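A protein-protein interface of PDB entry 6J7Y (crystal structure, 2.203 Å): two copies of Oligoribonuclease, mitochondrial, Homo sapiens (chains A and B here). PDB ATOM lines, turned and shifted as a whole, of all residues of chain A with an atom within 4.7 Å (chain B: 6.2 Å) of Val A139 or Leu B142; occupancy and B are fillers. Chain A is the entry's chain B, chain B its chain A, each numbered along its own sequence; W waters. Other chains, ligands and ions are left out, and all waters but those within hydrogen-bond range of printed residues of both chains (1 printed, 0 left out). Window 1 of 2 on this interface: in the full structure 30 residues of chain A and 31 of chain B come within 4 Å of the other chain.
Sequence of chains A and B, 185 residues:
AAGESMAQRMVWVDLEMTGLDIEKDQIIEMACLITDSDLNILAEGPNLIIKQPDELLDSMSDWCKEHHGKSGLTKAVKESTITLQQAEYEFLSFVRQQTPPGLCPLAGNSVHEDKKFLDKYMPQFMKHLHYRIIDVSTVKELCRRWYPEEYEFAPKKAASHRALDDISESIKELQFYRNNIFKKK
OG1 of Thr B138 sits at hydrogen-bond distance from N of Asp A135, 2.9 Å away.
O of Ile B133 lies within hydrogen-bond range of OG1 of Thr A138 (3.1 Å).
The backbone NH (N) of Ser A137 is in hydrogen-bond range of the side-chain carboxylate (OD1) of Asp A135, 2.9 Å away.
The side-chain hydroxyl (OG1) of Thr A138 sits at hydrogen-bond distance from the side-chain carboxylate (OD2) of Asp A135, at 3.0 Å.
NE of Arg B144 is in salt-bridge range of OE2 of Glu B141 (3.0 Å).
The side-chain carboxylate (OE1) of Glu B141 is in salt-bridge range of the guanidinium group (NE) of Arg B145 (2.9 Å).
Among the printed residues, pairs that only touch across the chains: Ile A134 with Glu B141, Phe A182 with Tyr B147, Ile A181 with Phe B182, Phe A182 with Ile B181, Asp A135 with Ile B133, Phe A182 with Phe B182, Leu A142 with Val B139, Val A139 with Leu B142, Met A10 with Arg B145 and Ile A134 with Thr B138.
Of chain B, only Leu B142 comes within 4 Å of Val A139.
Leu B142 touches one residue of chain A.
Of the printed residues of chain B, Ile A181 touches Phe B182 (3.5 Å).
Of the printed residues of chain A, Phe B182 touches Ile A181 (3.5 Å) and Phe A182 (3.6 Å).
Of the printed residues of chain A, Arg B145 touches Met A10.
Of the printed residues of chain B, Phe A182 touches Tyr B147 (3.4 Å), Ile B181 (3.5 Å) and Phe B182 (3.6 Å).
Of the printed residues of chain A, Thr B138 touches Ile A134 (3.8 Å) and Asp A135 (2.9 Å).
Cys B143 touches none of the printed residues of chain A.
Leu A174 touches none of the printed residues of chain B.
Hydrophobic or aromatic side chains of chain A that line the printed part of chain B: Met A10, Ile A134, Val A139, Leu A142, Ile A181 and Phe A182.
Of the 14 printed residues of chain B, 9 touch a printed residue of chain A.
Printed residues of chain B that touch a printed residue of chain A: Ile B133, Thr B138, Val B139, Glu B141, Leu B142, Arg B145, Tyr B147, Ile B181 and Phe B182.
Hydrophobic or aromatic side chains of chain B within 4 Å of the printed part of chain A: Ile B133, Val B139, Leu B142, Tyr B147 and Phe B182.
Among the printed residues, 12 pairs touch across the chains.
Val A139 touches Leu B142, and with the chains exchanged Leu A142 touches Val B139.
Ile A181 touches Phe B182, and with the chains exchanged Phe A182 touches Ile B181.
Phe B182 touches its own counterpart, Phe A182.
Positions printed for both chains: 137, 138, 139, 140, 141, 142, 143, 181 and 182.
Of the 12 pairs that touch across the chains among the printed residues, 5 have their exchanged pair printed and touching as well.
Water W1 bridges the side-chain carboxylate (OD2) of Asp A135 and the backbone NH (N) of Ile B133.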
ATOM      1  N   MET A  10     -18.941  -6.884   4.220  1.00  0.00           N
ATOM      2  CA  MET A  10     -18.559  -7.733   3.098  1.00  0.00           C
ATOM      3  C   MET A  10     -19.803  -8.238   2.377  1.00  0.00           C
ATOM      4  O   MET A  10     -20.802  -8.604   3.027  1.00  0.00           O
ATOM      5  CB  MET A  10     -17.735  -8.932   3.550  1.00  0.00           C
ATOM      6  CG  MET A  10     -16.430  -8.629   4.328  1.00  0.00           C
ATOM      7  SD  MET A  10     -15.713 -10.232   4.773  1.00  0.00           S
ATOM      8  CE  MET A  10     -14.394  -9.729   5.904  1.00  0.00           C
ATOM      9  N   ILE A 134     -12.400 -10.659  -1.435  1.00  0.00           N
ATOM     10  CA  ILE A 134     -11.980 -11.499  -0.330  1.00  0.00           C
ATOM     11  C   ILE A 134     -12.195 -12.934  -0.780  1.00  0.00           C
ATOM     12  O   ILE A 134     -13.320 -13.448  -0.722  1.00  0.00           O
ATOM     13  CB  ILE A 134     -12.758 -11.204   0.949  1.00  0.00           C
ATOM     14  CG1 ILE A 134     -12.547  -9.756   1.374  1.00  0.00           C
ATOM     15  CG2 ILE A 134     -12.365 -12.228   2.026  1.00  0.00           C
ATOM     16  CD1 ILE A 134     -11.238  -9.511   1.977  1.00  0.00           C
ATOM     17  N   ASP A 135     -11.108 -13.582  -1.181  1.00  0.00           N
ATOM     18  CA  ASP A 135     -11.118 -14.911  -1.783  1.00  0.00           C
ATOM     19  C   ASP A 135     -10.773 -15.920  -0.699  1.00  0.00           C
ATOM     20  O   ASP A 135      -9.614 -16.046  -0.299  1.00  0.00           O
ATOM     21  CB  ASP A 135     -10.125 -14.963  -2.943  1.00  0.00           C
ATOM     22  CG  ASP A 135      -9.977 -16.355  -3.538  1.00  0.00           C
ATOM     23  OD1 ASP A 135     -10.838 -17.231  -3.299  1.00  0.00           O
ATOM     24  OD2 ASP A 135      -8.972 -16.575  -4.243  1.00  0.00           O
ATOM     25  N   VAL A 136     -11.786 -16.641  -0.216  1.00  0.00           N
ATOM     26  CA  VAL A 136     -11.561 -17.632   0.831  1.00  0.00           C
ATOM     27  C   VAL A 136     -10.614 -18.729   0.339  1.00  0.00           C
ATOM     28  O   VAL A 136      -9.891 -19.346   1.135  1.00  0.00           O
ATOM     29  CB  VAL A 136     -12.929 -18.201   1.289  1.00  0.00           C
ATOM     30  CG1 VAL A 136     -12.761 -19.325   2.300  1.00  0.00           C
ATOM     31  CG2 VAL A 136     -13.807 -17.085   1.884  1.00  0.00           C
ATOM     32  N   SER A 137     -10.612 -18.995  -0.973  1.00  0.00           N
ATOM     33  CA  SER A 137      -9.769 -20.058  -1.511  1.00  0.00           C
ATOM     34  C   SER A 137      -8.285 -19.714  -1.434  1.00  0.00           C
ATOM     35  O   SER A 137      -7.456 -20.618  -1.308  1.00  0.00           O
ATOM     36  CB  SER A 137     -10.179 -20.371  -2.948  1.00  0.00           C
ATOM     37  OG  SER A 137     -11.170 -21.386  -2.938  1.00  0.00           O
ATOM     38  N   THR A 138      -7.931 -18.426  -1.487  1.00  0.00           N
ATOM     39  CA  THR A 138      -6.556 -18.022  -1.180  1.00  0.00           C
ATOM     40  C   THR A 138      -6.157 -18.456   0.229  1.00  0.00           C
ATOM     41  O   THR A 138      -5.065 -19.001   0.450  1.00  0.00           O
ATOM     42  CB  THR A 138      -6.416 -16.507  -1.311  1.00  0.00           C
ATOM     43  OG1 THR A 138      -6.433 -16.141  -2.689  1.00  0.00           O
ATOM     44  CG2 THR A 138      -5.131 -16.028  -0.640  1.00  0.00           C
ATOM     45  N   VAL A 139      -7.032 -18.204   1.205  1.00  0.00           N
ATOM     46  CA  VAL A 139      -6.727 -18.595   2.576  1.00  0.00           C
ATOM     47  C   VAL A 139      -6.657 -20.110   2.677  1.00  0.00           C
ATOM     48  O   VAL A 139      -5.799 -20.660   3.365  1.00  0.00           O
ATOM     49  CB  VAL A 139      -7.758 -17.986   3.550  1.00  0.00           C
ATOM     50  CG1 VAL A 139      -7.354 -18.249   5.013  1.00  0.00           C
ATOM     51  CG2 VAL A 139      -7.892 -16.464   3.313  1.00  0.00           C
ATOM     52  N   LYS A 140      -7.537 -20.808   1.962  1.00  0.00           N
ATOM     53  CA  LYS A 140      -7.498 -22.270   1.950  1.00  0.00           C
ATOM     54  C   LYS A 140      -6.164 -22.793   1.411  1.00  0.00           C
ATOM     55  O   LYS A 140      -5.568 -23.711   1.986  1.00  0.00           O
ATOM     56  CB  LYS A 140      -8.673 -22.789   1.113  1.00  0.00           C
ATOM     57  CG  LYS A 140      -8.659 -24.266   0.755  1.00  0.00           C
ATOM     58  CD  LYS A 140      -9.733 -24.536  -0.312  1.00  0.00           C
ATOM     59  CE  LYS A 140     -10.124 -26.015  -0.382  1.00  0.00           C
ATOM     60  NZ  LYS A 140     -11.130 -26.404   0.657  1.00  0.00           N
ATOM     61  N   GLU A 141      -5.689 -22.231   0.291  1.00  0.00           N
ATOM     62  CA  GLU A 141      -4.389 -22.631  -0.261  1.00  0.00           C
ATOM     63  C   GLU A 141      -3.260 -22.354   0.721  1.00  0.00           C
ATOM     64  O   GLU A 141      -2.360 -23.190   0.914  1.00  0.00           O
ATOM     65  CB  GLU A 141      -4.135 -21.887  -1.570  1.00  0.00           C
ATOM     66  CG  GLU A 141      -4.978 -22.420  -2.723  1.00  0.00           C
ATOM     67  CD  GLU A 141      -4.780 -23.924  -2.901  1.00  0.00           C
ATOM     68  OE1 GLU A 141      -3.626 -24.350  -3.132  1.00  0.00           O
ATOM     69  OE2 GLU A 141      -5.765 -24.677  -2.790  1.00  0.00           O
ATOM     70  N   LEU A 142      -3.317 -21.203   1.393  1.00  0.00           N
ATOM     71  CA  LEU A 142      -2.286 -20.886   2.375  1.00  0.00           C
ATOM     72  C   LEU A 142      -2.343 -21.836   3.568  1.00  0.00           C
ATOM     73  O   LEU A 142      -1.303 -22.281   4.053  1.00  0.00           O
ATOM     74  CB  LEU A 142      -2.425 -19.431   2.831  1.00  0.00           C
ATOM     75  CG  LEU A 142      -2.123 -18.425   1.714  1.00  0.00           C
ATOM     76  CD1 LEU A 142      -2.351 -17.011   2.220  1.00  0.00           C
ATOM     77  CD2 LEU A 142      -0.667 -18.592   1.201  1.00  0.00           C
ATOM     78  N   CYS A 143      -3.548 -22.125   4.076  1.00  0.00           N
ATOM     79  CA  CYS A 143      -3.706 -23.048   5.198  1.00  0.00           C
ATOM     80  C   CYS A 143      -3.218 -24.444   4.826  1.00  0.00           C
ATOM     81  O   CYS A 143      -2.563 -25.118   5.626  1.00  0.00           O
ATOM     82  CB  CYS A 143      -5.172 -23.098   5.621  1.00  0.00           C
ATOM     83  SG  CYS A 143      -5.540 -24.235   6.998  1.00  0.00           S
ATOM     84  N   LEU A 174     -13.992 -19.556   6.206  1.00  0.00           N
ATOM     85  CA  LEU A 174     -13.143 -18.428   6.574  1.00  0.00           C
ATOM     86  C   LEU A 174     -13.083 -18.268   8.089  1.00  0.00           C
ATOM     87  O   LEU A 174     -12.011 -18.010   8.656  1.00  0.00           O
ATOM     88  CB  LEU A 174     -13.630 -17.142   5.923  1.00  0.00           C
ATOM     89  CG  LEU A 174     -12.650 -15.998   6.205  1.00  0.00           C
ATOM     90  CD1 LEU A 174     -11.223 -16.384   5.757  1.00  0.00           C
ATOM     91  CD2 LEU A 174     -13.112 -14.709   5.517  1.00  0.00           C
ATOM     92  N   TYR A 177     -10.668 -20.734   9.536  1.00  0.00           N
ATOM     93  CA  TYR A 177      -9.293 -20.278   9.355  1.00  0.00           C
ATOM     94  C   TYR A 177      -8.950 -19.193  10.372  1.00  0.00           C
ATOM     95  O   TYR A 177      -7.903 -19.256  11.026  1.00  0.00           O
ATOM     96  CB  TYR A 177      -9.063 -19.772   7.928  1.00  0.00           C
ATOM     97  CG  TYR A 177      -9.241 -20.852   6.887  1.00  0.00           C
ATOM     98  CD1 TYR A 177      -8.765 -22.136   7.109  1.00  0.00           C
ATOM     99  CD2 TYR A 177      -9.889 -20.589   5.690  1.00  0.00           C
ATOM    100  CE1 TYR A 177      -8.931 -23.131   6.169  1.00  0.00           C
ATOM    101  CE2 TYR A 177     -10.059 -21.573   4.749  1.00  0.00           C
ATOM    102  CZ  TYR A 177      -9.585 -22.844   4.995  1.00  0.00           C
ATOM    103  OH  TYR A 177      -9.752 -23.827   4.044  1.00  0.00           O
ATOM    104  N   ILE A 181      -5.826 -20.531  12.392  1.00  0.00           N
ATOM    105  CA  ILE A 181      -4.484 -20.312  11.842  1.00  0.00           C
ATOM    106  C   ILE A 181      -4.037 -18.850  11.879  1.00  0.00           C
ATOM    107  O   ILE A 181      -2.887 -18.543  11.544  1.00  0.00           O
ATOM    108  CB  ILE A 181      -4.377 -20.860  10.410  1.00  0.00           C
ATOM    109  CG1 ILE A 181      -5.169 -19.987   9.436  1.00  0.00           C
ATOM    110  CG2 ILE A 181      -4.807 -22.360  10.375  1.00  0.00           C
ATOM    111  CD1 ILE A 181      -4.755 -20.174   7.971  1.00  0.00           C
ATOM    112  N   PHE A 182      -4.912 -17.937  12.278  1.00  0.00           N
ATOM    113  CA  PHE A 182      -4.507 -16.544  12.441  1.00  0.00           C
ATOM    114  C   PHE A 182      -4.124 -16.303  13.899  1.00  0.00           C
ATOM    115  O   PHE A 182      -4.630 -16.966  14.804  1.00  0.00           O
ATOM    116  CB  PHE A 182      -5.623 -15.587  12.001  1.00  0.00           C
ATOM    117  CG  PHE A 182      -5.730 -15.429  10.501  1.00  0.00           C
ATOM    118  CD1 PHE A 182      -6.348 -16.400   9.725  1.00  0.00           C
ATOM    119  CD2 PHE A 182      -5.195 -14.316   9.866  1.00  0.00           C
ATOM    120  CE1 PHE A 182      -6.428 -16.269   8.352  1.00  0.00           C
ATOM    121  CE2 PHE A 182      -5.290 -14.170   8.482  1.00  0.00           C
ATOM    122  CZ  PHE A 182      -5.906 -15.152   7.728  1.00  0.00           C
ATOM    123  N   ILE B 133      -6.133 -19.293  -7.044  1.00  0.00           N
ATOM    124  CA  ILE B 133      -5.081 -18.289  -7.030  1.00  0.00           C
ATOM    125  C   ILE B 133      -4.705 -18.035  -5.586  1.00  0.00           C
ATOM    126  O   ILE B 133      -5.434 -18.380  -4.655  1.00  0.00           O
ATOM    127  CB  ILE B 133      -5.482 -16.947  -7.682  1.00  0.00           C
ATOM    128  CG1 ILE B 133      -6.610 -16.303  -6.878  1.00  0.00           C
ATOM    129  CG2 ILE B 133      -5.862 -17.128  -9.146  1.00  0.00           C
ATOM    130  CD1 ILE B 133      -7.224 -15.095  -7.546  1.00  0.00           C
ATOM    131  N   SER B 137      -3.789  -9.658  -2.058  1.00  0.00           N
ATOM    132  CA  SER B 137      -4.707  -8.584  -1.677  1.00  0.00           C
ATOM    133  C   SER B 137      -5.820  -9.085  -0.775  1.00  0.00           C
ATOM    134  O   SER B 137      -6.305  -8.332   0.075  1.00  0.00           O
ATOM    135  CB  SER B 137      -5.310  -7.931  -2.917  1.00  0.00           C
ATOM    136  OG  SER B 137      -4.335  -7.122  -3.543  1.00  0.00           O
ATOM    137  N   THR B 138      -6.244 -10.337  -0.934  1.00  0.00           N
ATOM    138  CA  THR B 138      -7.184 -10.907   0.029  1.00  0.00           C
ATOM    139  C   THR B 138      -6.593 -10.873   1.430  1.00  0.00           C
ATOM    140  O   THR B 138      -7.244 -10.432   2.393  1.00  0.00           O
ATOM    141  CB  THR B 138      -7.532 -12.344  -0.358  1.00  0.00           C
ATOM    142  OG1 THR B 138      -8.463 -12.348  -1.446  1.00  0.00           O
ATOM    143  CG2 THR B 138      -8.125 -13.108   0.849  1.00  0.00           C
ATOM    144  N   VAL B 139      -5.341 -11.334   1.561  1.00  0.00           N
ATOM    145  CA  VAL B 139      -4.702 -11.366   2.872  1.00  0.00           C
ATOM    146  C   VAL B 139      -4.507  -9.949   3.383  1.00  0.00           C
ATOM    147  O   VAL B 139      -4.626  -9.683   4.583  1.00  0.00           O
ATOM    148  CB  VAL B 139      -3.370 -12.150   2.808  1.00  0.00           C
ATOM    149  CG1 VAL B 139      -2.718 -12.224   4.183  1.00  0.00           C
ATOM    150  CG2 VAL B 139      -3.606 -13.568   2.246  1.00  0.00           C
ATOM    151  N   LYS B 140      -4.204  -9.016   2.479  1.00  0.00           N
ATOM    152  CA  LYS B 140      -4.063  -7.613   2.863  1.00  0.00           C
ATOM    153  C   LYS B 140      -5.359  -7.071   3.439  1.00  0.00           C
ATOM    154  O   LYS B 140      -5.342  -6.376   4.464  1.00  0.00           O
ATOM    155  CB  LYS B 140      -3.619  -6.796   1.644  1.00  0.00           C
ATOM    156  CG  LYS B 140      -3.536  -5.299   1.825  1.00  0.00           C
ATOM    157  CD  LYS B 140      -3.182  -4.642   0.480  1.00  0.00           C
ATOM    158  CE  LYS B 140      -2.887  -3.143   0.609  1.00  0.00           C
ATOM    159  NZ  LYS B 140      -1.860  -2.838   1.651  1.00  0.00           N
ATOM    160  N   GLU B 141      -6.504  -7.409   2.810  1.00  0.00           N
ATOM    161  CA  GLU B 141      -7.797  -6.946   3.312  1.00  0.00           C
ATOM    162  C   GLU B 141      -8.101  -7.551   4.676  1.00  0.00           C
ATOM    163  O   GLU B 141      -8.612  -6.865   5.578  1.00  0.00           O
ATOM    164  CB  GLU B 141      -8.918  -7.300   2.323  1.00  0.00           C
ATOM    165  CG  GLU B 141      -9.329  -6.163   1.424  1.00  0.00           C
ATOM    166  CD  GLU B 141      -9.740  -4.935   2.224  1.00  0.00           C
ATOM    167  OE1 GLU B 141     -10.738  -4.997   2.978  1.00  0.00           O
ATOM    168  OE2 GLU B 141      -9.046  -3.918   2.121  1.00  0.00           O
ATOM    169  N   LEU B 142      -7.802  -8.842   4.843  1.00  0.00           N
ATOM    170  CA  LEU B 142      -7.964  -9.452   6.158  1.00  0.00           C
ATOM    171  C   LEU B 142      -7.060  -8.776   7.188  1.00  0.00           C
ATOM    172  O   LEU B 142      -7.485  -8.510   8.314  1.00  0.00           O
ATOM    173  CB  LEU B 142      -7.693 -10.959   6.084  1.00  0.00           C
ATOM    174  CG  LEU B 142      -8.654 -11.739   5.159  1.00  0.00           C
ATOM    175  CD1 LEU B 142      -8.391 -13.256   5.175  1.00  0.00           C
ATOM    176  CD2 LEU B 142     -10.121 -11.452   5.505  1.00  0.00           C
ATOM    177  N   CYS B 143      -5.813  -8.482   6.825  1.00  0.00           N
ATOM    178  CA  CYS B 143      -4.915  -7.806   7.758  1.00  0.00           C
ATOM    179  C   CYS B 143      -5.472  -6.446   8.179  1.00  0.00           C
ATOM    180  O   CYS B 143      -5.502  -6.115   9.370  1.00  0.00           O
ATOM    181  CB  CYS B 143      -3.537  -7.638   7.134  1.00  0.00           C
ATOM    182  SG  CYS B 143      -2.318  -6.984   8.306  1.00  0.00           S
ATOM    183  N   ARG B 144      -5.897  -5.642   7.204  1.00  0.00           N
ATOM    184  CA  ARG B 144      -6.487  -4.333   7.493  1.00  0.00           C
ATOM    185  C   ARG B 144      -7.655  -4.438   8.472  1.00  0.00           C
ATOM    186  O   ARG B 144      -7.770  -3.635   9.401  1.00  0.00           O
ATOM    187  CB  ARG B 144      -6.957  -3.684   6.191  1.00  0.00           C
ATOM    188  CG  ARG B 144      -7.247  -2.201   6.296  1.00  0.00           C
ATOM    189  CD  ARG B 144      -7.755  -1.651   4.965  1.00  0.00           C
ATOM    190  NE  ARG B 144      -9.056  -2.205   4.596  1.00  0.00           N
ATOM    191  CZ  ARG B 144     -10.214  -1.801   5.115  1.00  0.00           C
ATOM    192  NH1 ARG B 144     -10.233  -0.832   6.027  1.00  0.00           N
ATOM    193  NH2 ARG B 144     -11.356  -2.362   4.721  1.00  0.00           N
ATOM    194  N   ARG B 145      -8.523  -5.430   8.290  1.00  0.00           N
ATOM    195  CA  ARG B 145      -9.714  -5.518   9.128  1.00  0.00           C
ATOM    196  C   ARG B 145      -9.409  -6.096  10.505  1.00  0.00           C
ATOM    197  O   ARG B 145      -9.858  -5.574  11.536  1.00  0.00           O
ATOM    198  CB  ARG B 145     -10.763  -6.379   8.428  1.00  0.00           C
ATOM    199  CG  ARG B 145     -11.336  -5.750   7.173  1.00  0.00           C
ATOM    200  CD  ARG B 145     -12.145  -6.766   6.344  1.00  0.00           C
ATOM    201  NE  ARG B 145     -12.480  -6.162   5.051  1.00  0.00           N
ATOM    202  CZ  ARG B 145     -13.569  -5.434   4.854  1.00  0.00           C
ATOM    203  NH1 ARG B 145     -14.420  -5.247   5.850  1.00  0.00           N
ATOM    204  NH2 ARG B 145     -13.803  -4.893   3.676  1.00  0.00           N
ATOM    205  N   TRP B 146      -8.685  -7.203  10.532  1.00  0.00           N
ATOM    206  CA  TRP B 146      -8.493  -7.964  11.746  1.00  0.00           C
ATOM    207  C   TRP B 146      -7.207  -7.606  12.479  1.00  0.00           C
ATOM    208  O   TRP B 146      -7.101  -7.899  13.672  1.00  0.00           O
ATOM    209  CB  TRP B 146      -8.477  -9.463  11.424  1.00  0.00           C
ATOM    210  CG  TRP B 146      -9.716  -9.986  10.787  1.00  0.00           C
ATOM    211  CD1 TRP B 146     -10.931  -9.369  10.720  1.00  0.00           C
ATOM    212  CD2 TRP B 146      -9.872 -11.256  10.138  1.00  0.00           C
ATOM    213  NE1 TRP B 146     -11.828 -10.165  10.069  1.00  0.00           N
ATOM    214  CE2 TRP B 146     -11.210 -11.333   9.698  1.00  0.00           C
ATOM    215  CE3 TRP B 146      -9.009 -12.330   9.886  1.00  0.00           C
ATOM    216  CZ2 TRP B 146     -11.715 -12.443   9.017  1.00  0.00           C
ATOM    217  CZ3 TRP B 146      -9.514 -13.452   9.197  1.00  0.00           C
ATOM    218  CH2 TRP B 146     -10.848 -13.490   8.770  1.00  0.00           C
ATOM    219  N   TYR B 147      -6.216  -7.008  11.804  1.00  0.00           N
ATOM    220  CA  TYR B 147      -4.936  -6.685  12.445  1.00  0.00           C
ATOM    221  C   TYR B 147      -4.493  -5.274  12.076  1.00  0.00           C
ATOM    222  O   TYR B 147      -3.425  -5.074  11.481  1.00  0.00           O
ATOM    223  CB  TYR B 147      -3.878  -7.724  12.060  1.00  0.00           C
ATOM    224  CG  TYR B 147      -4.257  -9.091  12.558  1.00  0.00           C
ATOM    225  CD1 TYR B 147      -3.863  -9.523  13.825  1.00  0.00           C
ATOM    226  CD2 TYR B 147      -5.062  -9.929  11.792  1.00  0.00           C
ATOM    227  CE1 TYR B 147      -4.248 -10.767  14.300  1.00  0.00           C
ATOM    228  CE2 TYR B 147      -5.449 -11.181  12.260  1.00  0.00           C
ATOM    229  CZ  TYR B 147      -5.030 -11.591  13.510  1.00  0.00           C
ATOM    230  OH  TYR B 147      -5.412 -12.820  13.987  1.00  0.00           O
ATOM    231  N   ILE B 181       0.610 -11.922  11.339  1.00  0.00           N
ATOM    232  CA  ILE B 181      -0.802 -12.122  11.642  1.00  0.00           C
ATOM    233  C   ILE B 181      -1.232 -13.578  11.570  1.00  0.00           C
ATOM    234  O   ILE B 181      -2.390 -13.876  11.861  1.00  0.00           O
ATOM    235  CB  ILE B 181      -1.706 -11.255  10.746  1.00  0.00           C
ATOM    236  CG1 ILE B 181      -1.699 -11.772   9.305  1.00  0.00           C
ATOM    237  CG2 ILE B 181      -1.290  -9.784  10.840  1.00  0.00           C
ATOM    238  CD1 ILE B 181      -2.757 -11.069   8.432  1.00  0.00           C
ATOM    239  N   PHE B 182      -0.351 -14.498  11.199  1.00  0.00           N
ATOM    240  CA  PHE B 182      -0.665 -15.918  11.248  1.00  0.00           C
ATOM    241  C   PHE B 182      -0.083 -16.556  12.513  1.00  0.00           C
ATOM    242  O   PHE B 182       0.947 -16.130  13.034  1.00  0.00           O
ATOM    243  CB  PHE B 182      -0.143 -16.631   9.992  1.00  0.00           C
ATOM    244  CG  PHE B 182      -1.008 -16.416   8.757  1.00  0.00           C
ATOM    245  CD1 PHE B 182      -0.898 -15.253   8.004  1.00  0.00           C
ATOM    246  CD2 PHE B 182      -1.932 -17.380   8.357  1.00  0.00           C
ATOM    247  CE1 PHE B 182      -1.705 -15.052   6.862  1.00  0.00           C
ATOM    248  CE2 PHE B 182      -2.732 -17.191   7.215  1.00  0.00           C
ATOM    249  CZ  PHE B 182      -2.617 -16.035   6.474  1.00  0.00           C
HETATM  250  O   HOH W   1      -8.450 -18.843  -5.485  1.00  0.00           O
